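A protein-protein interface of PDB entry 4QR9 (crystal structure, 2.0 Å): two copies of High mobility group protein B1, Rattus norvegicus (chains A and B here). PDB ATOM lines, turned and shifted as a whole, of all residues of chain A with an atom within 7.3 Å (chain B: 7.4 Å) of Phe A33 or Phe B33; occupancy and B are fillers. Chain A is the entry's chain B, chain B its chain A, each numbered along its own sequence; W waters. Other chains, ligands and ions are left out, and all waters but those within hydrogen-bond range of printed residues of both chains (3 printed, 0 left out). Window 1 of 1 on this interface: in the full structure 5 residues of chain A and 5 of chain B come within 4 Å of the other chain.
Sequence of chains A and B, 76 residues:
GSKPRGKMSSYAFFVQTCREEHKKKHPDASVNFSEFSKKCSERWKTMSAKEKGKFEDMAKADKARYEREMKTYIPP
The side-chain hydroxyl (OG) of Ser B30 lies within hydrogen-bond range of the side-chain amide nitrogen (ND2) of Asn A32, at 3.4 Å. The side-chain amide nitrogen (ND2) of Asn B32 lies within hydrogen-bond range of the side-chain hydroxyl (OG) of Ser A30 (3.1 Å).
Phe A33 touches Phe B33.
Ser A30 touches Asn B32, and with the chains exchanged Asn A32 touches Ser B30. Phe B33 touches its own counterpart, Phe A33. 10 positions are printed for both chains.
N of Glu A35 lies within hydrogen-bond range of OD1 of Asn A32, 3.1 Å away. The side-chain amide oxygen (OD1) of Asn B32 is in hydrogen-bond range of the backbone NH (N) of Glu B35 (3.1 Å). N of Ser B34 sits close to OD1 of Asn B32 (3.4 Å). OD1 of Asn A32 sits close to N of Ser A34 (3.3 Å).
Water W3 lies within hydrogen-bond range of the backbone carbonyl oxygen of Val B31 (2.7 Å), the backbone carbonyl oxygen of Val A31 (2.8 Å), the backbone NH of Phe B33 (2.8 Å) and the backbone NH of Phe A33 (2.9 Å). Water W1 lies within hydrogen-bond range of the side-chain amide oxygen (OD1) of Asn B32, the backbone carbonyl oxygen (O) of Val A31, the backbone NH (N) of Ser B34 and the backbone NH (N) of Phe B33. Water W2 lies within hydrogen-bond range of O of Val B31, OD1 of Asn A32, N of Ser A34 and N of Phe A33.
Of the printed residues of chain B, Asn A32 touches Ser B30. Phe A33 touches just one residue of chain B: Phe B33 (3.5 Å). Printed residues of chain A within 4 Å of Ser B30: Asn A32. Of the printed residues of chain A, Asn B32 touches Ser A30. Phe B33 touches just one residue of chain A: Phe A33 (3.5 Å). The nearest residue of chain B that does not touch Phe A33 is Val B31 (4.7 Å). The nearest residue of chain A that does not touch Phe B33 is Val A31 (4.7 Å). The nearest printed residue of chain A that does not touch Asn B32 is Val A31 (4.7 Å).
Of the 10 printed residues of chain A, 3 touch a printed residue of chain B. Hydrophobic or aromatic side chains of chain B within 4 Å of the printed part of chain A: Phe B33. Among the printed residues, 3 pairs touch across the chains. Among the printed residues, no Asp or Glu carboxylate lies within 4 Å of a Lys or Arg side-chain nitrogen of the other chain.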
ATOM      1  N   SER A  30       8.150  14.999 -31.234  1.00  0.00           N
ATOM      2  CA  SER A  30       8.347  13.778 -30.477  1.00  0.00           C
ATOM      3  C   SER A  30       6.993  13.000 -30.537  1.00  0.00           C
ATOM      4  O   SER A  30       5.919  13.582 -30.772  1.00  0.00           O
ATOM      5  CB  SER A  30       8.827  14.059 -29.068  1.00  0.00           C
ATOM      6  OG  SER A  30       7.730  14.258 -28.220  1.00  0.00           O
ATOM      7  N   VAL A  31       7.074  11.685 -30.474  1.00  0.00           N
ATOM      8  CA  VAL A  31       5.864  10.849 -30.543  1.00  0.00           C
ATOM      9  C   VAL A  31       5.064  10.963 -29.232  1.00  0.00           C
ATOM     10  O   VAL A  31       5.616  10.780 -28.138  1.00  0.00           O
ATOM     11  CB  VAL A  31       6.211   9.386 -30.800  1.00  0.00           C
ATOM     12  CG1 VAL A  31       4.930   8.522 -30.928  1.00  0.00           C
ATOM     13  CG2 VAL A  31       6.998   9.247 -32.080  1.00  0.00           C
ATOM     14  N   ASN A  32       3.793  11.289 -29.335  1.00  0.00           N
ATOM     15  CA  ASN A  32       2.863  11.234 -28.180  1.00  0.00           C
ATOM     16  C   ASN A  32       2.300   9.810 -28.254  1.00  0.00           C
ATOM     17  O   ASN A  32       1.449   9.494 -29.097  1.00  0.00           O
ATOM     18  CB  ASN A  32       1.801  12.340 -28.317  1.00  0.00           C
ATOM     19  CG  ASN A  32       0.630  12.185 -27.332  1.00  0.00           C
ATOM     20  OD1 ASN A  32       0.464  11.160 -26.698  1.00  0.00           O
ATOM     21  ND2 ASN A  32      -0.210  13.230 -27.229  1.00  0.00           N
ATOM     22  N   PHE A  33       2.855   8.904 -27.475  1.00  0.00           N
ATOM     23  CA  PHE A  33       2.494   7.462 -27.608  1.00  0.00           C
ATOM     24  C   PHE A  33       1.019   7.178 -27.495  1.00  0.00           C
ATOM     25  O   PHE A  33       0.429   6.430 -28.258  1.00  0.00           O
ATOM     26  CB  PHE A  33       3.279   6.626 -26.587  1.00  0.00           C
ATOM     27  CG  PHE A  33       4.638   6.176 -27.060  1.00  0.00           C
ATOM     28  CD1 PHE A  33       5.607   7.118 -27.548  1.00  0.00           C
ATOM     29  CD2 PHE A  33       5.023   4.845 -26.935  1.00  0.00           C
ATOM     30  CE1 PHE A  33       6.846   6.711 -27.869  1.00  0.00           C
ATOM     31  CE2 PHE A  33       6.296   4.454 -27.285  1.00  0.00           C
ATOM     32  CZ  PHE A  33       7.211   5.370 -27.705  1.00  0.00           C
ATOM     33  N   SER A  34       0.365   7.819 -26.554  1.00  0.00           N
ATOM     34  CA  SER A  34      -1.053   7.648 -26.376  1.00  0.00           C
ATOM     35  C   SER A  34      -1.867   8.084 -27.642  1.00  0.00           C
ATOM     36  O   SER A  34      -2.701   7.333 -28.206  1.00  0.00           O
ATOM     37  CB  SER A  34      -1.481   8.457 -25.137  1.00  0.00           C
ATOM     38  OG  SER A  34      -2.888   8.491 -25.182  1.00  0.00           O
ATOM     39  N   GLU A  35      -1.575   9.267 -28.122  1.00  0.00           N
ATOM     40  CA  GLU A  35      -2.274   9.789 -29.259  1.00  0.00           C
ATOM     41  C   GLU A  35      -1.924   9.077 -30.552  1.00  0.00           C
ATOM     42  O   GLU A  35      -2.807   8.772 -31.352  1.00  0.00           O
ATOM     43  CB  GLU A  35      -2.073  11.262 -29.392  1.00  0.00           C
ATOM     44  CG  GLU A  35      -3.036  11.860 -30.403  1.00  0.00           C
ATOM     45  CD  GLU A  35      -4.547  11.576 -30.082  1.00  0.00           C
ATOM     46  OE1 GLU A  35      -5.308  11.391 -31.064  1.00  0.00           O
ATOM     47  OE2 GLU A  35      -4.986  11.496 -28.876  1.00  0.00           O
ATOM     48  N   PHE A  36      -0.672   8.695 -30.711  1.00  0.00           N
ATOM     49  CA  PHE A  36      -0.199   7.942 -31.845  1.00  0.00           C
ATOM     50  C   PHE A  36      -0.901   6.633 -31.947  1.00  0.00           C
ATOM     51  O   PHE A  36      -1.308   6.232 -33.023  1.00  0.00           O
ATOM     52  CB  PHE A  36       1.338   7.734 -31.722  1.00  0.00           C
ATOM     53  CG  PHE A  36       1.932   6.842 -32.731  1.00  0.00           C
ATOM     54  CD1 PHE A  36       2.147   7.291 -34.066  1.00  0.00           C
ATOM     55  CD2 PHE A  36       2.251   5.529 -32.446  1.00  0.00           C
ATOM     56  CE1 PHE A  36       2.706   6.434 -35.007  1.00  0.00           C
ATOM     57  CE2 PHE A  36       2.816   4.680 -33.393  1.00  0.00           C
ATOM     58  CZ  PHE A  36       3.063   5.127 -34.662  1.00  0.00           C
ATOM     59  N   SER A  37      -1.037   5.915 -30.793  1.00  0.00           N
ATOM     60  CA  SER A  37      -1.690   4.641 -30.809  1.00  0.00           C
ATOM     61  C   SER A  37      -3.162   4.779 -31.269  1.00  0.00           C
ATOM     62  O   SER A  37      -3.666   3.906 -32.020  1.00  0.00           O
ATOM     63  CB  SER A  37      -1.660   4.002 -29.394  1.00  0.00           C
ATOM     64  OG  SER A  37      -2.337   2.796 -29.423  1.00  0.00           O
ATOM     65  N   LYS A  38      -3.872   5.768 -30.740  1.00  0.00           N
ATOM     66  CA  LYS A  38      -5.255   6.022 -31.114  1.00  0.00           C
ATOM     67  C   LYS A  38      -5.406   6.363 -32.608  1.00  0.00           C
ATOM     68  O   LYS A  38      -6.309   5.833 -33.244  1.00  0.00           O
ATOM     69  CB  LYS A  38      -5.854   7.135 -30.304  1.00  0.00           C
ATOM     70  CG  LYS A  38      -5.998   6.810 -28.835  1.00  0.00           C
ATOM     71  CD  LYS A  38      -6.640   7.992 -28.111  1.00  0.00           C
ATOM     72  CE  LYS A  38      -6.303   7.940 -26.617  1.00  0.00           C
ATOM     73  NZ  LYS A  38      -7.250   8.660 -25.715  1.00  0.00           N
ATOM     74  N   LYS A  39      -4.524   7.205 -33.156  1.00  0.00           N
ATOM     75  CA  LYS A  39      -4.542   7.498 -34.588  1.00  0.00           C
ATOM     76  C   LYS A  39      -4.198   6.343 -35.484  1.00  0.00           C
ATOM     77  O   LYS A  39      -4.821   6.164 -36.546  1.00  0.00           O
ATOM     78  CB  LYS A  39      -3.579   8.651 -34.917  1.00  0.00           C
ATOM     79  CG  LYS A  39      -4.100   9.931 -34.336  1.00  0.00           C
ATOM     80  CD  LYS A  39      -3.146  11.095 -34.558  1.00  0.00           C
ATOM     81  CE  LYS A  39      -3.876  12.378 -34.165  1.00  0.00           C
ATOM     82  NZ  LYS A  39      -3.003  13.570 -34.259  1.00  0.00           N
ATOM     83  N   SER B  30      -0.411  14.474 -21.159  1.00  0.00           N
ATOM     84  CA  SER B  30      -0.023  13.195 -21.690  1.00  0.00           C
ATOM     85  C   SER B  30       1.506  12.985 -21.378  1.00  0.00           C
ATOM     86  O   SER B  30       2.291  13.931 -21.225  1.00  0.00           O
ATOM     87  CB  SER B  30      -0.373  13.072 -23.176  1.00  0.00           C
ATOM     88  OG  SER B  30       0.673  13.603 -23.956  1.00  0.00           O
ATOM     89  N   VAL B  31       1.893  11.735 -21.214  1.00  0.00           N
ATOM     90  CA  VAL B  31       3.293  11.390 -20.975  1.00  0.00           C
ATOM     91  C   VAL B  31       4.084  11.510 -22.300  1.00  0.00           C
ATOM     92  O   VAL B  31       3.681  10.925 -23.325  1.00  0.00           O
ATOM     93  CB  VAL B  31       3.410   9.965 -20.434  1.00  0.00           C
ATOM     94  CG1 VAL B  31       4.858   9.622 -20.197  1.00  0.00           C
ATOM     95  CG2 VAL B  31       2.608   9.825 -19.168  1.00  0.00           C
ATOM     96  N   ASN B  32       5.193  12.231 -22.303  1.00  0.00           N
ATOM     97  CA  ASN B  32       6.158  12.184 -23.459  1.00  0.00           C
ATOM     98  C   ASN B  32       7.097  11.016 -23.128  1.00  0.00           C
ATOM     99  O   ASN B  32       7.974  11.129 -22.255  1.00  0.00           O
ATOM    100  CB  ASN B  32       6.877  13.517 -23.591  1.00  0.00           C
ATOM    101  CG  ASN B  32       7.995  13.525 -24.641  1.00  0.00           C
ATOM    102  OD1 ASN B  32       8.591  12.513 -24.998  1.00  0.00           O
ATOM    103  ND2 ASN B  32       8.273  14.727 -25.158  1.00  0.00           N
ATOM    104  N   PHE B  33       6.891   9.861 -23.756  1.00  0.00           N
ATOM    105  CA  PHE B  33       7.571   8.645 -23.331  1.00  0.00           C
ATOM    106  C   PHE B  33       9.086   8.767 -23.408  1.00  0.00           C
ATOM    107  O   PHE B  33       9.864   8.341 -22.510  1.00  0.00           O
ATOM    108  CB  PHE B  33       7.108   7.438 -24.149  1.00  0.00           C
ATOM    109  CG  PHE B  33       5.870   6.703 -23.632  1.00  0.00           C
ATOM    110  CD1 PHE B  33       4.679   7.377 -23.383  1.00  0.00           C
ATOM    111  CD2 PHE B  33       5.861   5.337 -23.592  1.00  0.00           C
ATOM    112  CE1 PHE B  33       3.567   6.697 -22.914  1.00  0.00           C
ATOM    113  CE2 PHE B  33       4.757   4.643 -23.159  1.00  0.00           C
ATOM    114  CZ  PHE B  33       3.621   5.332 -22.830  1.00  0.00           C
ATOM    115  N   SER B  34       9.567   9.342 -24.502  1.00  0.00           N
ATOM    116  CA  SER B  34      10.996   9.513 -24.669  1.00  0.00           C
ATOM    117  C   SER B  34      11.641  10.434 -23.580  1.00  0.00           C
ATOM    118  O   SER B  34      12.603  10.032 -22.877  1.00  0.00           O
ATOM    119  CB  SER B  34      11.233  10.140 -26.083  1.00  0.00           C
ATOM    120  OG  SER B  34      12.567  10.588 -26.067  1.00  0.00           O
ATOM    121  N   GLU B  35      11.070  11.608 -23.370  1.00  0.00           N
ATOM    122  CA  GLU B  35      11.546  12.481 -22.317  1.00  0.00           C
ATOM    123  C   GLU B  35      11.364  11.885 -20.903  1.00  0.00           C
ATOM    124  O   GLU B  35      12.215  12.029 -20.088  1.00  0.00           O
ATOM    125  CB  GLU B  35      10.848  13.833 -22.365  1.00  0.00           C
ATOM    126  CG  GLU B  35      11.216  14.858 -21.297  1.00  0.00           C
ATOM    127  CD  GLU B  35      10.274  16.082 -21.406  1.00  0.00           C
ATOM    128  OE1 GLU B  35      10.371  16.807 -22.431  1.00  0.00           O
ATOM    129  OE2 GLU B  35       9.399  16.297 -20.519  1.00  0.00           O
ATOM    130  N   PHE B  36      10.253  11.207 -20.663  1.00  0.00           N
ATOM    131  CA  PHE B  36       9.943  10.627 -19.367  1.00  0.00           C
ATOM    132  C   PHE B  36      10.980   9.595 -19.007  1.00  0.00           C
ATOM    133  O   PHE B  36      11.455   9.549 -17.858  1.00  0.00           O
ATOM    134  CB  PHE B  36       8.527  10.025 -19.369  1.00  0.00           C
ATOM    135  CG  PHE B  36       8.183   9.179 -18.147  1.00  0.00           C
ATOM    136  CD1 PHE B  36       7.759   9.797 -16.963  1.00  0.00           C
ATOM    137  CD2 PHE B  36       8.199   7.805 -18.203  1.00  0.00           C
ATOM    138  CE1 PHE B  36       7.457   9.044 -15.827  1.00  0.00           C
ATOM    139  CE2 PHE B  36       7.913   7.045 -17.059  1.00  0.00           C
ATOM    140  CZ  PHE B  36       7.489   7.660 -15.895  1.00  0.00           C
ATOM    141  N   SER B  37      11.313   8.731 -19.951  1.00  0.00           N
ATOM    142  CA  SER B  37      12.293   7.698 -19.717  1.00  0.00           C
ATOM    143  C   SER B  37      13.650   8.316 -19.357  1.00  0.00           C
ATOM    144  O   SER B  37      14.330   7.798 -18.455  1.00  0.00           O
ATOM    145  CB  SER B  37      12.443   6.811 -20.965  1.00  0.00           C
ATOM    146  OG  SER B  37      13.467   5.858 -20.816  1.00  0.00           O
ATOM    147  N   LYS B  38      14.075   9.322 -20.139  1.00  0.00           N
ATOM    148  CA  LYS B  38      15.343   9.981 -19.888  1.00  0.00           C
ATOM    149  C   LYS B  38      15.391  10.626 -18.519  1.00  0.00           C
ATOM    150  O   LYS B  38      16.410  10.491 -17.819  1.00  0.00           O
ATOM    151  CB  LYS B  38      15.651  11.011 -20.909  1.00  0.00           C
ATOM    152  CG  LYS B  38      15.875  10.454 -22.303  1.00  0.00           C
ATOM    153  CD  LYS B  38      16.148  11.655 -23.256  1.00  0.00           C
ATOM    154  CE  LYS B  38      15.827  11.398 -24.706  1.00  0.00           C
ATOM    155  NZ  LYS B  38      16.892  10.515 -25.204  1.00  0.00           N
ATOM    156  N   LYS B  39      14.334  11.329 -18.127  1.00  0.00           N
ATOM    157  CA  LYS B  39      14.222  11.926 -16.798  1.00  0.00           C
ATOM    158  C   LYS B  39      14.230  10.928 -15.644  1.00  0.00           C
ATOM    159  O   LYS B  39      14.876  11.176 -14.625  1.00  0.00           O
ATOM    160  CB  LYS B  39      12.959  12.810 -16.667  1.00  0.00           C
ATOM    161  CG  LYS B  39      13.094  14.060 -17.540  1.00  0.00           C
ATOM    162  CD  LYS B  39      11.860  14.935 -17.493  1.00  0.00           C
ATOM    163  CE  LYS B  39      12.228  16.247 -18.200  1.00  0.00           C
ATOM    164  NZ  LYS B  39      11.069  17.150 -18.284  1.00  0.00           N
HETATM  165  O   HOH W   1       8.159  10.447 -26.806  1.00  0.00           O
HETATM  166  O   HOH W   2       1.462   9.644 -24.462  1.00  0.00           O
HETATM  167  O   HOH W   3       4.736  10.006 -25.615  1.00  0.00           O
